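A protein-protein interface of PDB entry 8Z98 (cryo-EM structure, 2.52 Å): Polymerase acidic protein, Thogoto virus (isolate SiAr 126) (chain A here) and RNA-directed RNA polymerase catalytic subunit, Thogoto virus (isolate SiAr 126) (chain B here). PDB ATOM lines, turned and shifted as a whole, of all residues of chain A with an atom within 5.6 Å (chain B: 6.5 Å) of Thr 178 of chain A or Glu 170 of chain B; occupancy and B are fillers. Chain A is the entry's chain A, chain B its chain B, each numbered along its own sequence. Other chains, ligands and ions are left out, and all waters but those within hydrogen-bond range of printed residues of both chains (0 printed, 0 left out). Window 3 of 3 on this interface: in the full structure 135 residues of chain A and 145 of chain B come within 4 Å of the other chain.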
ATOM      1  N   VAL A 175      -5.235  14.028  24.888  1.00  0.00           N
ATOM      2  CA  VAL A 175      -5.043  13.070  23.806  1.00  0.00           C
ATOM      3  C   VAL A 175      -5.708  11.765  24.216  1.00  0.00           C
ATOM      4  O   VAL A 175      -5.440  11.242  25.304  1.00  0.00           O
ATOM      5  CB  VAL A 175      -3.552  12.851  23.495  1.00  0.00           C
ATOM      6  CG1 VAL A 175      -3.386  11.817  22.395  1.00  0.00           C
ATOM      7  CG2 VAL A 175      -2.894  14.161  23.108  1.00  0.00           C
ATOM      8  N   GLY A 176      -6.570  11.240  23.350  1.00  0.00           N
ATOM      9  CA  GLY A 176      -7.298  10.028  23.651  1.00  0.00           C
ATOM     10  C   GLY A 176      -6.456   8.780  23.477  1.00  0.00           C
ATOM     11  O   GLY A 176      -5.296   8.816  23.071  1.00  0.00           O
ATOM     12  N   THR A 177      -7.073   7.644  23.803  1.00  0.00           N
ATOM     13  CA  THR A 177      -6.360   6.372  23.751  1.00  0.00           C
ATOM     14  C   THR A 177      -6.069   5.949  22.316  1.00  0.00           C
ATOM     15  O   THR A 177      -4.982   5.438  22.025  1.00  0.00           O
ATOM     16  CB  THR A 177      -7.165   5.292  24.471  1.00  0.00           C
ATOM     17  OG1 THR A 177      -8.527   5.334  24.031  1.00  0.00           O
ATOM     18  CG2 THR A 177      -7.119   5.513  25.975  1.00  0.00           C
ATOM     19  N   THR A 178      -7.025   6.148  21.407  1.00  0.00           N
ATOM     20  CA  THR A 178      -6.852   5.683  20.034  1.00  0.00           C
ATOM     21  C   THR A 178      -5.761   6.470  19.316  1.00  0.00           C
ATOM     22  O   THR A 178      -4.907   5.892  18.630  1.00  0.00           O
ATOM     23  CB  THR A 178      -8.175   5.788  19.278  1.00  0.00           C
ATOM     24  OG1 THR A 178      -9.222   5.212  20.068  1.00  0.00           O
ATOM     25  CG2 THR A 178      -8.085   5.040  17.967  1.00  0.00           C
ATOM     26  N   PHE A 179      -5.774   7.796  19.464  1.00  0.00           N
ATOM     27  CA  PHE A 179      -4.714   8.611  18.882  1.00  0.00           C
ATOM     28  C   PHE A 179      -3.369   8.299  19.520  1.00  0.00           C
ATOM     29  O   PHE A 179      -2.335   8.348  18.847  1.00  0.00           O
ATOM     30  CB  PHE A 179      -5.058  10.093  19.030  1.00  0.00           C
ATOM     31  CG  PHE A 179      -4.159  11.008  18.250  1.00  0.00           C
ATOM     32  CD1 PHE A 179      -3.792  10.701  16.952  1.00  0.00           C
ATOM     33  CD2 PHE A 179      -3.701  12.189  18.808  1.00  0.00           C
ATOM     34  CE1 PHE A 179      -2.971  11.545  16.233  1.00  0.00           C
ATOM     35  CE2 PHE A 179      -2.882  13.037  18.093  1.00  0.00           C
ATOM     36  CZ  PHE A 179      -2.517  12.715  16.804  1.00  0.00           C
ATOM     37  N   ARG A 180      -3.364   7.961  20.812  1.00  0.00           N
ATOM     38  CA  ARG A 180      -2.125   7.561  21.470  1.00  0.00           C
ATOM     39  C   ARG A 180      -1.575   6.269  20.875  1.00  0.00           C
ATOM     40  O   ARG A 180      -0.365   6.144  20.648  1.00  0.00           O
ATOM     41  CB  ARG A 180      -2.369   7.410  22.971  1.00  0.00           C
ATOM     42  CG  ARG A 180      -1.113   7.354  23.807  1.00  0.00           C
ATOM     43  CD  ARG A 180      -1.443   7.428  25.286  1.00  0.00           C
ATOM     44  NE  ARG A 180      -2.228   8.613  25.608  1.00  0.00           N
ATOM     45  CZ  ARG A 180      -1.765   9.660  26.278  1.00  0.00           C
ATOM     46  NH1 ARG A 180      -0.520   9.701  26.721  1.00  0.00           N
ATOM     47  NH2 ARG A 180      -2.573  10.689  26.512  1.00  0.00           N
ATOM     48  N   THR A 181      -2.451   5.294  20.616  1.00  0.00           N
ATOM     49  CA  THR A 181      -2.011   4.055  19.985  1.00  0.00           C
ATOM     50  C   THR A 181      -1.496   4.310  18.575  1.00  0.00           C
ATOM     51  O   THR A 181      -0.513   3.696  18.146  1.00  0.00           O
ATOM     52  CB  THR A 181      -3.149   3.033  19.958  1.00  0.00           C
ATOM     53  OG1 THR A 181      -4.273   3.582  19.261  1.00  0.00           O
ATOM     54  CG2 THR A 181      -3.561   2.653  21.369  1.00  0.00           C
ATOM     55  N   LEU A 182      -2.157   5.203  17.835  1.00  0.00           N
ATOM     56  CA  LEU A 182      -1.657   5.570  16.512  1.00  0.00           C
ATOM     57  C   LEU A 182      -0.273   6.203  16.601  1.00  0.00           C
ATOM     58  O   LEU A 182       0.609   5.902  15.790  1.00  0.00           O
ATOM     59  CB  LEU A 182      -2.633   6.520  15.822  1.00  0.00           C
ATOM     60  CG  LEU A 182      -3.965   5.931  15.364  1.00  0.00           C
ATOM     61  CD1 LEU A 182      -4.877   7.024  14.838  1.00  0.00           C
ATOM     62  CD2 LEU A 182      -3.735   4.873  14.304  1.00  0.00           C
ATOM     63  N   LEU A 183      -0.068   7.085  17.581  1.00  0.00           N
ATOM     64  CA  LEU A 183       1.226   7.740  17.738  1.00  0.00           C
ATOM     65  C   LEU A 183       2.318   6.738  18.084  1.00  0.00           C
ATOM     66  O   LEU A 183       3.437   6.823  17.565  1.00  0.00           O
ATOM     67  CB  LEU A 183       1.136   8.818  18.818  1.00  0.00           C
ATOM     68  CG  LEU A 183       0.501  10.154  18.435  1.00  0.00           C
ATOM     69  CD1 LEU A 183       0.301  11.011  19.670  1.00  0.00           C
ATOM     70  CD2 LEU A 183       1.353  10.877  17.412  1.00  0.00           C
ATOM     71  N   ILE B 165      -7.978  18.664  16.123  1.00  0.00           N
ATOM     72  CA  ILE B 165      -7.306  17.619  15.349  1.00  0.00           C
ATOM     73  C   ILE B 165      -7.193  16.338  16.170  1.00  0.00           C
ATOM     74  O   ILE B 165      -7.500  15.235  15.695  1.00  0.00           O
ATOM     75  CB  ILE B 165      -5.923  18.107  14.881  1.00  0.00           C
ATOM     76  CG1 ILE B 165      -6.062  19.309  13.945  1.00  0.00           C
ATOM     77  CG2 ILE B 165      -5.170  16.986  14.202  1.00  0.00           C
ATOM     78  CD1 ILE B 165      -6.640  18.965  12.599  1.00  0.00           C
ATOM     79  N   ALA B 166      -6.757  16.471  17.425  1.00  0.00           N
ATOM     80  CA  ALA B 166      -6.616  15.305  18.289  1.00  0.00           C
ATOM     81  C   ALA B 166      -7.956  14.630  18.543  1.00  0.00           C
ATOM     82  O   ALA B 166      -8.013  13.403  18.686  1.00  0.00           O
ATOM     83  CB  ALA B 166      -5.961  15.708  19.609  1.00  0.00           C
ATOM     84  N   ASP B 167      -9.040  15.406  18.605  1.00  0.00           N
ATOM     85  CA  ASP B 167     -10.357  14.822  18.831  1.00  0.00           C
ATOM     86  C   ASP B 167     -10.877  14.121  17.583  1.00  0.00           C
ATOM     87  O   ASP B 167     -11.475  13.044  17.676  1.00  0.00           O
ATOM     88  CB  ASP B 167     -11.339  15.899  19.287  1.00  0.00           C
ATOM     89  CG  ASP B 167     -11.066  16.373  20.701  1.00  0.00           C
ATOM     90  OD1 ASP B 167     -10.530  15.579  21.502  1.00  0.00           O
ATOM     91  OD2 ASP B 167     -11.389  17.538  21.014  1.00  0.00           O
ATOM     92  N   VAL B 168     -10.672  14.718  16.405  1.00  0.00           N
ATOM     93  CA  VAL B 168     -11.142  14.085  15.181  1.00  0.00           C
ATOM     94  C   VAL B 168     -10.332  12.836  14.871  1.00  0.00           C
ATOM     95  O   VAL B 168     -10.814  11.945  14.161  1.00  0.00           O
ATOM     96  CB  VAL B 168     -11.118  15.072  13.996  1.00  0.00           C
ATOM     97  CG1 VAL B 168      -9.697  15.333  13.533  1.00  0.00           C
ATOM     98  CG2 VAL B 168     -11.981  14.560  12.850  1.00  0.00           C
ATOM     99  N   MET B 169      -9.110  12.734  15.400  1.00  0.00           N
ATOM    100  CA  MET B 169      -8.367  11.491  15.253  1.00  0.00           C
ATOM    101  C   MET B 169      -8.972  10.334  16.040  1.00  0.00           C
ATOM    102  O   MET B 169      -8.566   9.186  15.828  1.00  0.00           O
ATOM    103  CB  MET B 169      -6.909  11.693  15.671  1.00  0.00           C
ATOM    104  CG  MET B 169      -6.064  12.506  14.691  1.00  0.00           C
ATOM    105  SD  MET B 169      -6.258  12.180  12.919  1.00  0.00           S
ATOM    106  CE  MET B 169      -6.322  10.388  12.834  1.00  0.00           C
ATOM    107  N   GLU B 170      -9.925  10.597  16.932  1.00  0.00           N
ATOM    108  CA  GLU B 170     -10.531   9.563  17.761  1.00  0.00           C
ATOM    109  C   GLU B 170     -11.792   8.967  17.151  1.00  0.00           C
ATOM    110  O   GLU B 170     -12.423   8.115  17.785  1.00  0.00           O
ATOM    111  CB  GLU B 170     -10.865  10.127  19.145  1.00  0.00           C
ATOM    112  CG  GLU B 170      -9.803  11.048  19.701  1.00  0.00           C
ATOM    113  CD  GLU B 170      -8.622  10.310  20.288  1.00  0.00           C
ATOM    114  OE1 GLU B 170      -8.615   9.062  20.264  1.00  0.00           O
ATOM    115  OE2 GLU B 170      -7.681  10.987  20.752  1.00  0.00           O
ATOM    116  N   LEU B 171     -12.178   9.389  15.954  1.00  0.00           N
ATOM    117  CA  LEU B 171     -13.428   8.965  15.342  1.00  0.00           C
ATOM    118  C   LEU B 171     -13.183   7.835  14.352  1.00  0.00           C
ATOM    119  O   LEU B 171     -12.220   7.869  13.580  1.00  0.00           O
ATOM    120  CB  LEU B 171     -14.110  10.137  14.635  1.00  0.00           C
ATOM    121  CG  LEU B 171     -14.539  11.297  15.532  1.00  0.00           C
ATOM    122  CD1 LEU B 171     -15.028  12.458  14.690  1.00  0.00           C
ATOM    123  CD2 LEU B 171     -15.610  10.853  16.512  1.00  0.00           C
ATOM    124  N   ASP B 172     -14.059   6.830  14.387  1.00  0.00           N
ATOM    125  CA  ASP B 172     -13.956   5.726  13.439  1.00  0.00           C
ATOM    126  C   ASP B 172     -14.150   6.208  12.007  1.00  0.00           C
ATOM    127  O   ASP B 172     -13.420   5.793  11.100  1.00  0.00           O
ATOM    128  CB  ASP B 172     -14.986   4.646  13.775  1.00  0.00           C
ATOM    129  CG  ASP B 172     -14.677   3.925  15.070  1.00  0.00           C
ATOM    130  OD1 ASP B 172     -13.486   3.819  15.427  1.00  0.00           O
ATOM    131  OD2 ASP B 172     -15.627   3.458  15.731  1.00  0.00           O
ATOM    132  N   ARG B 216     -10.292   6.329   9.952  1.00  0.00           N
ATOM    133  CA  ARG B 216      -9.225   6.673  10.883  1.00  0.00           C
ATOM    134  C   ARG B 216      -7.858   6.360  10.290  1.00  0.00           C
ATOM    135  O   ARG B 216      -6.918   7.149  10.432  1.00  0.00           O
ATOM    136  CB  ARG B 216      -9.405   5.946  12.212  1.00  0.00           C
ATOM    137  CG  ARG B 216      -8.279   6.236  13.188  1.00  0.00           C
ATOM    138  CD  ARG B 216      -8.431   5.464  14.476  1.00  0.00           C
ATOM    139  NE  ARG B 216      -9.705   5.735  15.130  1.00  0.00           N
ATOM    140  CZ  ARG B 216     -10.623   4.816  15.387  1.00  0.00           C
ATOM    141  NH1 ARG B 216     -10.448   3.550  15.047  1.00  0.00           N
ATOM    142  NH2 ARG B 216     -11.747   5.176  16.001  1.00  0.00           N
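OE1 of Glu 170 of chain B lies within hydrogen-bond range of N of Phe 179 of chain A (3.2 Å). The backbone NH (N) of Gly 176 of chain A is in hydrogen-bond range of the side-chain carboxylate (OE2) of Glu 170 of chain B (2.8 Å).
The backbone carbonyl oxygen (O) of Thr 178 of chain A lies within hydrogen-bond range of the side-chain hydroxyl (OG1) of Thr 181 of chain A, at 2.5 Å. OD1 of Asp 172 of chain B lies within salt-bridge range of NH1 of Arg 216 of chain B (3.1 Å).
Thr 178 of chain A touches Glu 170 of chain B. Thr 178 of chain A touches Arg 216 of chain B (CG2 to NE, 3.3 Å). CD1 of Phe 179 of chain A touches CB of Met 169 of chain B, at 3.5 Å. CD1 of Leu 182 of chain A touches CG of Arg 216 of chain B (3.9 Å).
Printed residues of chain B within 4 Å of Gly 176 of chain A: Glu 170. Of chain B, only Glu 170 and Arg 216 come within 4 Å of Thr 178 of chain A. Of the printed residues of chain B, Phe 179 of chain A touches Met 169 (3.5 Å) and Glu 170 (3.2 Å). Thr 181 of chain A touches none of the printed residues of chain B. Val 168 of chain B touches none of the printed residues of chain A. Of chain A, only Gly 176 (2.8 Å), Thr 178 (3.4 Å) and Phe 179 (3.2 Å) come within 4 Å of Glu 170 of chain B. Of the printed residues of chain A, Arg 216 of chain B touches Thr 178 and Leu 182. The nearest residue of chain B that does not touch Thr 178 of chain A is Met 169 of chain B (4.7 Å). The nearest printed residue of chain B that does not touch Gly 176 of chain A is Ala 166 of chain B (5.3 Å).
Of the 9 printed residues of chain A, 4 touch a printed residue of chain B. Along chain A the printed residues that touch a printed residue of chain B span positions 176 to 182. Printed residues of chain B that touch a printed residue of chain A: Met 169, Glu 170 and Arg 216. Along chain B the printed residues that touch a printed residue of chain A span positions 169 to 216. Among the printed residues, 6 pairs touch across the chains.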
